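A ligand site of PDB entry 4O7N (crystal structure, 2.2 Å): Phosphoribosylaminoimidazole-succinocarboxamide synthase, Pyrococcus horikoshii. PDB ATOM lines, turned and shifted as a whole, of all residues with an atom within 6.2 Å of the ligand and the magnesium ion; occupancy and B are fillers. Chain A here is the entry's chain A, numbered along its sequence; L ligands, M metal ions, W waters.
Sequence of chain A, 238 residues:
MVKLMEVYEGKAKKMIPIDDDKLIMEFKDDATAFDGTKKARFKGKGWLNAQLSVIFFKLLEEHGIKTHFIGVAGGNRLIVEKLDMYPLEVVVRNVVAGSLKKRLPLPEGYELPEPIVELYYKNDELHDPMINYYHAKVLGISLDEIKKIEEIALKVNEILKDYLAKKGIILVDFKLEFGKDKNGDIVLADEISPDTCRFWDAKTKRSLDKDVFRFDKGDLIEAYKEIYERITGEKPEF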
ATOM      1  N   TYR A   8     -17.988  -6.814 -11.851  1.00  0.00           N
ATOM      2  CA  TYR A   8     -18.292  -5.807 -10.842  1.00  0.00           C
ATOM      3  C   TYR A   8     -19.660  -6.124 -10.235  1.00  0.00           C
ATOM      4  O   TYR A   8     -20.648  -6.269 -10.962  1.00  0.00           O
ATOM      5  CB  TYR A   8     -18.266  -4.390 -11.419  1.00  0.00           C
ATOM      6  CG  TYR A   8     -18.679  -3.319 -10.426  1.00  0.00           C
ATOM      7  CD1 TYR A   8     -19.992  -2.831 -10.400  1.00  0.00           C
ATOM      8  CD2 TYR A   8     -17.759  -2.802  -9.504  1.00  0.00           C
ATOM      9  CE1 TYR A   8     -20.374  -1.859  -9.477  1.00  0.00           C
ATOM     10  CE2 TYR A   8     -18.132  -1.829  -8.581  1.00  0.00           C
ATOM     11  CZ  TYR A   8     -19.434  -1.356  -8.573  1.00  0.00           C
ATOM     12  OH  TYR A   8     -19.807  -0.401  -7.659  1.00  0.00           O
ATOM     13  N   GLU A   9     -19.719  -6.249  -8.912  1.00  0.00           N
ATOM     14  CA  GLU A   9     -20.978  -6.474  -8.200  1.00  0.00           C
ATOM     15  C   GLU A   9     -21.384  -5.228  -7.399  1.00  0.00           C
ATOM     16  O   GLU A   9     -20.821  -4.960  -6.332  1.00  0.00           O
ATOM     17  CB  GLU A   9     -20.888  -7.719  -7.299  1.00  0.00           C
ATOM     18  N   GLY A  10     -22.361  -4.482  -7.916  1.00  0.00           N
ATOM     19  CA  GLY A  10     -22.906  -3.310  -7.212  1.00  0.00           C
ATOM     20  C   GLY A  10     -24.072  -3.698  -6.310  1.00  0.00           C
ATOM     21  O   GLY A  10     -24.462  -4.859  -6.264  1.00  0.00           O
ATOM     22  N   LYS A  11     -24.620  -2.709  -5.597  1.00  0.00           N
ATOM     23  CA  LYS A  11     -25.753  -2.914  -4.681  1.00  0.00           C
ATOM     24  C   LYS A  11     -26.981  -3.582  -5.319  1.00  0.00           C
ATOM     25  O   LYS A  11     -27.708  -4.348  -4.671  1.00  0.00           O
ATOM     26  CB  LYS A  11     -26.184  -1.587  -4.042  1.00  0.00           C
ATOM     27  CG  LYS A  11     -25.184  -0.996  -3.046  1.00  0.00           C
ATOM     28  CD  LYS A  11     -25.569   0.420  -2.607  1.00  0.00           C
ATOM     29  CE  LYS A  11     -25.151   1.468  -3.637  1.00  0.00           C
ATOM     30  N   ALA A  12     -27.210  -3.305  -6.607  1.00  0.00           N
ATOM     31  CA  ALA A  12     -28.424  -3.764  -7.285  1.00  0.00           C
ATOM     32  C   ALA A  12     -28.192  -4.590  -8.564  1.00  0.00           C
ATOM     33  O   ALA A  12     -29.085  -5.327  -9.003  1.00  0.00           O
ATOM     34  CB  ALA A  12     -29.328  -2.568  -7.586  1.00  0.00           C
ATOM     35  N   LYS A  13     -27.016  -4.440  -9.171  1.00  0.00           N
ATOM     36  CA  LYS A  13     -26.711  -5.089 -10.448  1.00  0.00           C
ATOM     37  C   LYS A  13     -25.269  -5.623 -10.472  1.00  0.00           C
ATOM     38  O   LYS A  13     -24.405  -5.124  -9.738  1.00  0.00           O
ATOM     39  CB  LYS A  13     -26.951  -4.137 -11.634  1.00  0.00           C
ATOM     40  CG  LYS A  13     -28.269  -3.359 -11.563  1.00  0.00           C
ATOM     41  CD  LYS A  13     -28.560  -2.486 -12.768  1.00  0.00           C
ATOM     42  CE  LYS A  13     -27.657  -1.254 -12.875  1.00  0.00           C
ATOM     43  NZ  LYS A  13     -27.813  -0.258 -11.778  1.00  0.00           N
ATOM     44  N   LYS A  14     -25.019  -6.629 -11.303  1.00  0.00           N
ATOM     45  CA  LYS A  14     -23.648  -7.028 -11.641  1.00  0.00           C
ATOM     46  C   LYS A  14     -23.302  -6.698 -13.110  1.00  0.00           C
ATOM     47  O   LYS A  14     -24.137  -6.872 -14.004  1.00  0.00           O
ATOM     48  CB  LYS A  14     -23.330  -8.496 -11.258  1.00  0.00           C
ATOM     49  CG  LYS A  14     -24.072  -9.566 -12.038  1.00  0.00           C
ATOM     50  N   MET A  15     -22.089  -6.204 -13.331  1.00  0.00           N
ATOM     51  CA  MET A  15     -21.635  -5.832 -14.664  1.00  0.00           C
ATOM     52  C   MET A  15     -20.571  -6.816 -15.125  1.00  0.00           C
ATOM     53  O   MET A  15     -19.473  -6.861 -14.579  1.00  0.00           O
ATOM     54  CB  MET A  15     -21.070  -4.392 -14.666  1.00  0.00           C
ATOM     55  CG  MET A  15     -21.958  -3.375 -13.960  1.00  0.00           C
ATOM     56  SD  MET A  15     -23.568  -3.134 -14.758  1.00  0.00           S
ATOM     57  CE  MET A  15     -23.082  -2.140 -16.171  1.00  0.00           C
ATOM     58  N   LEU A  23     -20.772  -4.781 -22.188  1.00  0.00           N
ATOM     59  CA  LEU A  23     -20.959  -5.324 -20.855  1.00  0.00           C
ATOM     60  C   LEU A  23     -22.283  -6.031 -20.765  1.00  0.00           C
ATOM     61  O   LEU A  23     -23.212  -5.733 -21.527  1.00  0.00           O
ATOM     62  CB  LEU A  23     -20.952  -4.215 -19.808  1.00  0.00           C
ATOM     63  CG  LEU A  23     -19.730  -3.327 -19.609  1.00  0.00           C
ATOM     64  CD1 LEU A  23     -20.093  -2.239 -18.606  1.00  0.00           C
ATOM     65  CD2 LEU A  23     -18.523  -4.139 -19.141  1.00  0.00           C
ATOM     66  N   MET A  25     -25.232  -6.259 -18.147  1.00  0.00           N
ATOM     67  CA  MET A  25     -25.797  -5.672 -16.942  1.00  0.00           C
ATOM     68  C   MET A  25     -26.854  -6.630 -16.400  1.00  0.00           C
ATOM     69  O   MET A  25     -27.925  -6.800 -17.007  1.00  0.00           O
ATOM     70  CB  MET A  25     -26.378  -4.294 -17.231  1.00  0.00           C
ATOM     71  CG  MET A  25     -26.932  -3.587 -15.999  1.00  0.00           C
ATOM     72  SD  MET A  25     -27.196  -1.829 -16.292  1.00  0.00           S
ATOM     73  CE  MET A  25     -28.512  -1.838 -17.509  1.00  0.00           C
ATOM     74  N   HIS A  68     -26.938   3.395 -23.593  1.00  0.00           N
ATOM     75  CA  HIS A  68     -26.015   2.275 -23.667  1.00  0.00           C
ATOM     76  C   HIS A  68     -26.679   0.958 -24.065  1.00  0.00           C
ATOM     77  O   HIS A  68     -25.992  -0.042 -24.243  1.00  0.00           O
ATOM     78  CB  HIS A  68     -25.224   2.154 -22.363  1.00  0.00           C
ATOM     79  CG  HIS A  68     -26.046   1.703 -21.181  1.00  0.00           C
ATOM     80  ND1 HIS A  68     -25.488   1.175 -20.064  1.00  0.00           N
ATOM     81  CD2 HIS A  68     -27.421   1.681 -20.963  1.00  0.00           C
ATOM     82  CE1 HIS A  68     -26.441   0.851 -19.180  1.00  0.00           C
ATOM     83  NE2 HIS A  68     -27.635   1.175 -19.724  1.00  0.00           N
ATOM     84  N   VAL A  80     -25.047  -4.066 -22.871  1.00  0.00           N
ATOM     85  CA  VAL A  80     -24.933  -2.609 -22.878  1.00  0.00           C
ATOM     86  C   VAL A  80     -23.536  -2.181 -23.328  1.00  0.00           C
ATOM     87  O   VAL A  80     -22.542  -2.882 -23.080  1.00  0.00           O
ATOM     88  CB  VAL A  80     -25.271  -1.982 -21.490  1.00  0.00           C
ATOM     89  CG1 VAL A  80     -26.725  -2.257 -21.077  1.00  0.00           C
ATOM     90  CG2 VAL A  80     -24.311  -2.441 -20.406  1.00  0.00           C
ATOM     91  N   GLU A  81     -23.453  -1.006 -23.958  1.00  0.00           N
ATOM     92  CA  GLU A  81     -22.175  -0.442 -24.366  1.00  0.00           C
ATOM     93  C   GLU A  81     -21.354  -0.084 -23.146  1.00  0.00           C
ATOM     94  O   GLU A  81     -21.875   0.475 -22.177  1.00  0.00           O
ATOM     95  CB  GLU A  81     -22.406   0.801 -25.239  1.00  0.00           C
ATOM     96  CG  GLU A  81     -21.192   1.255 -26.028  1.00  0.00           C
ATOM     97  CD  GLU A  81     -21.454   2.534 -26.816  1.00  0.00           C
ATOM     98  OE1 GLU A  81     -22.577   3.072 -26.759  1.00  0.00           O
ATOM     99  OE2 GLU A  81     -20.522   3.006 -27.482  1.00  0.00           O
ATOM    100  N   LYS A  82     -20.068  -0.401 -23.177  1.00  0.00           N
ATOM    101  CA  LYS A  82     -19.153  -0.014 -22.107  1.00  0.00           C
ATOM    102  C   LYS A  82     -18.784   1.447 -22.306  1.00  0.00           C
ATOM    103  O   LYS A  82     -18.455   1.880 -23.400  1.00  0.00           O
ATOM    104  CB  LYS A  82     -17.907  -0.893 -22.108  1.00  0.00           C
ATOM    105  CG  LYS A  82     -16.977  -0.641 -20.926  1.00  0.00           C
ATOM    106  CD  LYS A  82     -15.688  -1.445 -21.034  1.00  0.00           C
ATOM    107  CE  LYS A  82     -14.861  -1.293 -19.782  1.00  0.00           C
ATOM    108  NZ  LYS A  82     -13.476  -1.827 -19.964  1.00  0.00           N
ATOM    109  N   LEU A  83     -18.864   2.218 -21.230  1.00  0.00           N
ATOM    110  CA  LEU A  83     -18.638   3.641 -21.328  1.00  0.00           C
ATOM    111  C   LEU A  83     -17.662   4.081 -20.275  1.00  0.00           C
ATOM    112  O   LEU A  83     -17.493   3.452 -19.243  1.00  0.00           O
ATOM    113  CB  LEU A  83     -19.939   4.410 -21.127  1.00  0.00           C
ATOM    114  CG  LEU A  83     -21.084   4.160 -22.090  1.00  0.00           C
ATOM    115  CD1 LEU A  83     -22.377   4.737 -21.504  1.00  0.00           C
ATOM    116  CD2 LEU A  83     -20.786   4.750 -23.453  1.00  0.00           C
ATOM    117  N   ASP A  84     -17.047   5.215 -20.540  1.00  0.00           N
ATOM    118  CA  ASP A  84     -16.255   5.895 -19.562  1.00  0.00           C
ATOM    119  C   ASP A  84     -17.217   6.819 -18.759  1.00  0.00           C
ATOM    120  O   ASP A  84     -17.649   7.869 -19.243  1.00  0.00           O
ATOM    121  CB  ASP A  84     -15.187   6.669 -20.319  1.00  0.00           C
ATOM    122  CG  ASP A  84     -14.360   7.514 -19.425  1.00  0.00           C
ATOM    123  OD1 ASP A  84     -14.399   7.309 -18.187  1.00  0.00           O
ATOM    124  OD2 ASP A  84     -13.674   8.401 -19.980  1.00  0.00           O
ATOM    125  N   MET A  85     -17.569   6.378 -17.559  1.00  0.00           N
ATOM    126  CA  MET A  85     -18.656   6.964 -16.772  1.00  0.00           C
ATOM    127  C   MET A  85     -18.286   8.300 -16.138  1.00  0.00           C
ATOM    128  O   MET A  85     -17.183   8.469 -15.641  1.00  0.00           O
ATOM    129  CB  MET A  85     -19.115   6.001 -15.667  1.00  0.00           C
ATOM    130  CG  MET A  85     -19.747   4.692 -16.149  1.00  0.00           C
ATOM    131  SD  MET A  85     -21.264   4.883 -17.138  1.00  0.00           S
ATOM    132  CE  MET A  85     -22.358   5.613 -15.899  1.00  0.00           C
ATOM    133  N   GLU A  89     -24.644  11.421 -10.401  1.00  0.00           N
ATOM    134  CA  GLU A  89     -26.050  11.046 -10.439  1.00  0.00           C
ATOM    135  C   GLU A  89     -26.832  12.312 -10.791  1.00  0.00           C
ATOM    136  O   GLU A  89     -26.710  13.325 -10.091  1.00  0.00           O
ATOM    137  CB  GLU A  89     -26.498  10.459  -9.102  1.00  0.00           C
ATOM    138  CG  GLU A  89     -25.817   9.115  -8.792  1.00  0.00           C
ATOM    139  CD  GLU A  89     -26.004   8.612  -7.360  1.00  0.00           C
ATOM    140  OE1 GLU A  89     -25.429   7.543  -7.017  1.00  0.00           O
ATOM    141  OE2 GLU A  89     -26.731   9.246  -6.561  1.00  0.00           O
ATOM    142  N   LYS A 122     -20.869  11.241  -7.318  1.00  0.00           N
ATOM    143  CA  LYS A 122     -20.793   9.853  -6.824  1.00  0.00           C
ATOM    144  C   LYS A 122     -19.512   9.608  -6.059  1.00  0.00           C
ATOM    145  O   LYS A 122     -18.441   9.510  -6.659  1.00  0.00           O
ATOM    146  CB  LYS A 122     -20.886   8.853  -7.975  1.00  0.00           C
ATOM    147  CG  LYS A 122     -22.276   8.742  -8.563  1.00  0.00           C
ATOM    148  CD  LYS A 122     -22.311   7.692  -9.659  1.00  0.00           C
ATOM    149  CE  LYS A 122     -22.096   6.306  -9.082  1.00  0.00           C
ATOM    150  NZ  LYS A 122     -22.624   5.295 -10.027  1.00  0.00           N
ATOM    151  N   GLU A 177     -27.624   8.282 -14.953  1.00  0.00           N
ATOM    152  CA  GLU A 177     -26.163   8.280 -15.012  1.00  0.00           C
ATOM    153  C   GLU A 177     -25.762   8.327 -16.476  1.00  0.00           C
ATOM    154  O   GLU A 177     -26.541   7.897 -17.350  1.00  0.00           O
ATOM    155  CB  GLU A 177     -25.577   7.031 -14.356  1.00  0.00           C
ATOM    156  CG  GLU A 177     -25.860   6.919 -12.854  1.00  0.00           C
ATOM    157  CD  GLU A 177     -25.041   5.823 -12.193  1.00  0.00           C
ATOM    158  OE1 GLU A 177     -24.188   5.183 -12.868  1.00  0.00           O
ATOM    159  OE2 GLU A 177     -25.240   5.594 -10.993  1.00  0.00           O
ATOM    160  N   LEU A 188     -26.519   7.955 -22.252  1.00  0.00           N
ATOM    161  CA  LEU A 188     -27.299   7.637 -21.070  1.00  0.00           C
ATOM    162  C   LEU A 188     -27.061   6.179 -20.684  1.00  0.00           C
ATOM    163  O   LEU A 188     -27.088   5.294 -21.552  1.00  0.00           O
ATOM    164  CB  LEU A 188     -28.790   7.859 -21.337  1.00  0.00           C
ATOM    165  CG  LEU A 188     -29.760   7.540 -20.194  1.00  0.00           C
ATOM    166  CD1 LEU A 188     -29.516   8.537 -19.085  1.00  0.00           C
ATOM    167  CD2 LEU A 188     -31.178   7.680 -20.680  1.00  0.00           C
ATOM    168  N   ALA A 189     -26.822   5.938 -19.400  1.00  0.00           N
ATOM    169  CA  ALA A 189     -26.323   4.646 -18.946  1.00  0.00           C
ATOM    170  C   ALA A 189     -27.156   4.079 -17.778  1.00  0.00           C
ATOM    171  O   ALA A 189     -28.344   4.439 -17.632  1.00  0.00           O
ATOM    172  CB  ALA A 189     -24.838   4.760 -18.567  1.00  0.00           C
ATOM    173  N   ASP A 190     -26.557   3.196 -16.982  1.00  0.00           N
ATOM    174  CA  ASP A 190     -27.192   2.581 -15.810  1.00  0.00           C
ATOM    175  C   ASP A 190     -28.586   2.005 -16.116  1.00  0.00           C
ATOM    176  O   ASP A 190     -28.749   1.261 -17.085  1.00  0.00           O
ATOM    177  CB  ASP A 190     -27.229   3.574 -14.643  1.00  0.00           C
ATOM    178  CG  ASP A 190     -27.399   2.888 -13.291  1.00  0.00           C
ATOM    179  OD1 ASP A 190     -28.328   3.257 -12.564  1.00  0.00           O
ATOM    180  OD2 ASP A 190     -26.631   1.968 -12.958  1.00  0.00           O
ATOM    181  N   GLU A 191     -29.597   2.357 -15.309  1.00  0.00           N
ATOM    182  CA  GLU A 191     -30.916   1.731 -15.426  1.00  0.00           C
ATOM    183  C   GLU A 191     -32.000   2.773 -15.350  1.00  0.00           C
ATOM    184  O   GLU A 191     -31.740   3.901 -14.924  1.00  0.00           O
ATOM    185  CB  GLU A 191     -31.127   0.661 -14.311  1.00  0.00           C
ATOM    186  CG  GLU A 191     -31.346   1.241 -12.898  1.00  0.00           C
ATOM    187  CD  GLU A 191     -31.596   0.168 -11.843  1.00  0.00           C
ATOM    188  OE1 GLU A 191     -32.727  -0.350 -11.754  1.00  0.00           O
ATOM    189  OE2 GLU A 191     -30.656  -0.148 -11.090  1.00  0.00           O
HETATM  190  P1  LIG L   1     -23.613   0.669  -7.559  1.00  0.00           P
HETATM  191  O1  LIG L   1     -24.413   1.845  -8.068  1.00  0.00           O
HETATM  192  O2  LIG L   1     -24.209   0.017  -6.336  1.00  0.00           O
HETATM  193  O3  LIG L   1     -22.129   0.952  -7.497  1.00  0.00           O
HETATM  194  P2  LIG L   1     -25.002  -1.012  -9.457  1.00  0.00           P
HETATM  195  O4  LIG L   1     -25.518  -2.215  -8.698  1.00  0.00           O
HETATM  196  O5  LIG L   1     -25.978   0.105  -9.754  1.00  0.00           O
HETATM  197  O6  LIG L   1     -23.668  -0.457  -8.727  1.00  0.00           O
HETATM  198  O7  LIG L   1     -24.403  -1.586 -10.844  1.00  0.00           O
HETATM  199  C1  LIG L   1     -24.086  -0.745 -11.970  1.00  0.00           C
HETATM  200  C2  LIG L   1     -22.656  -0.175 -11.945  1.00  0.00           C
HETATM  201  O8  LIG L   1     -22.166  -0.008 -13.290  1.00  0.00           O
HETATM  202  C3  LIG L   1     -22.604   1.229 -11.376  1.00  0.00           C
HETATM  203  O9  LIG L   1     -21.292   1.422 -10.839  1.00  0.00           O
HETATM  204  C4  LIG L   1     -22.804   2.114 -12.606  1.00  0.00           C
HETATM  205  O10 LIG L   1     -22.345   3.452 -12.427  1.00  0.00           O
HETATM  206  C5  LIG L   1     -21.995   1.375 -13.645  1.00  0.00           C
HETATM  207  N1  LIG L   1     -22.485   1.491 -15.033  1.00  0.00           N
HETATM  208  C6  LIG L   1     -23.765   1.606 -15.448  1.00  0.00           C
HETATM  209  N2  LIG L   1     -23.846   1.644 -16.796  1.00  0.00           N
HETATM  210  C7  LIG L   1     -22.578   1.520 -17.280  1.00  0.00           C
HETATM  211  C8  LIG L   1     -21.891   1.481 -18.599  1.00  0.00           C
HETATM  212  N3  LIG L   1     -22.586   1.560 -19.754  1.00  0.00           N
HETATM  213  N4  LIG L   1     -20.542   1.369 -18.638  1.00  0.00           N
HETATM  214  C9  LIG L   1     -19.796   1.285 -17.518  1.00  0.00           C
HETATM  215  N5  LIG L   1     -20.341   1.303 -16.295  1.00  0.00           N
HETATM  216  C10 LIG L   1     -21.684   1.419 -16.108  1.00  0.00           C
HETATM  217 MG    MG M   1     -26.355   2.088  -8.752  1.00  0.00          MG
HETATM  218  O   HOH W   1     -19.778   4.259 -12.554  1.00  0.00           O
HETATM  219  O   HOH W   2     -25.464   2.838 -10.621  1.00  0.00           O
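N of Lys 11 is in hydrogen-bond range of O2 of the ligand (2.9 Å).
A nitrogen (N3) of the ligand is in hydrogen-bond range of a ring nitrogen (ND1) of His 68 (2.9 Å).
O4 of the ligand sits at hydrogen-bond distance from N of Ala 12, at 2.9 Å.
The side-chain amino group of Lys 13 sits close to an oxygen (O5) of the ligand.
The backbone carbonyl oxygen (O) of Glu 81 lies within hydrogen-bond range of a nitrogen (N3) of the ligand, 2.7 Å away.
The side-chain hydroxyl (OH) of Tyr 8 lies within hydrogen-bond range of an oxygen (O3) of the ligand (2.7 Å).
N2 of the ligand lies within hydrogen-bond range of N of Asp 190 (3.1 Å).
N of Lys 13 lies within hydrogen-bond range of O4 of the ligand (2.7 Å).
An oxygen (O10) of the ligand is in hydrogen-bond range of the side-chain amino group (NZ) of Lys 122 (3.0 Å).
The backbone NH (N) of Leu 83 lies within hydrogen-bond range of a nitrogen (N4) of the ligand (3.2 Å).
O10 of the ligand is in hydrogen-bond range of OE1 of Glu 177, at 2.6 Å.
Water W2 lies within hydrogen-bond range of OD2 of Asp 190 (2.8 Å) and OE2 of Glu 177 (2.8 Å).
O8 of the ligand lies close to SD of Met 15, 3.7 Å away.
A nitrogen (N5) of the ligand lies close to the side-chain sulfur (SD) of Met 85 (3.8 Å).
Gly 10 touches the ligand (C to O4, 3.2 Å).
Leu 23 touches the ligand.
CA of Lys 82 touches N4 of the ligand, 3.98 Å away.
Ala 189 touches the ligand (CB to N2, 3.7 Å).
Hydrophobic or aromatic side chains within 4 Å of the ligand: Tyr 8, Ala 12, Met 15, Leu 23, His 68, Leu 83, Met 85 and Ala 189.
The side-chain amino group (NZ) of Lys 13 lies within salt-bridge range of the side-chain carboxylate (OE2) of Glu 191, at 2.9 Å.
The backbone carbonyl oxygen (O) of Asp 190 lies within hydrogen-bond range of a ring nitrogen (NE2) of His 68 (2.9 Å).
The backbone NH (N) of Ala 189 lies within hydrogen-bond range of the backbone carbonyl oxygen (O) of Glu 177, at 2.8 Å.
The backbone carbonyl oxygen (O) of His 68 lies within hydrogen-bond range of the backbone NH (N) of Glu 81, at 2.7 Å.
The backbone carbonyl oxygen of Leu 188 lies within hydrogen-bond range of the backbone NH of His 68 (2.8 Å).
The backbone NH (N) of Leu 23 is in hydrogen-bond range of the backbone carbonyl oxygen (O) of Val 80, 2.7 Å away.
OD2 of Asp 190 lies within salt-bridge range of NZ of Lys 13, 2.8 Å away.
O of Tyr 8 is in hydrogen-bond range of N of Met 15, 2.8 Å away.
No residue comes within 4 Å of the magnesium ion.
An oxygen (O1) of the ligand binds the magnesium ion.
The magnesium ion is bound by water W2 (2.2 Å).
The magnesium ion is bound by an oxygen (O5) of the ligand (2.3 Å).
The magnesium ion has three donor atoms within binding distance.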
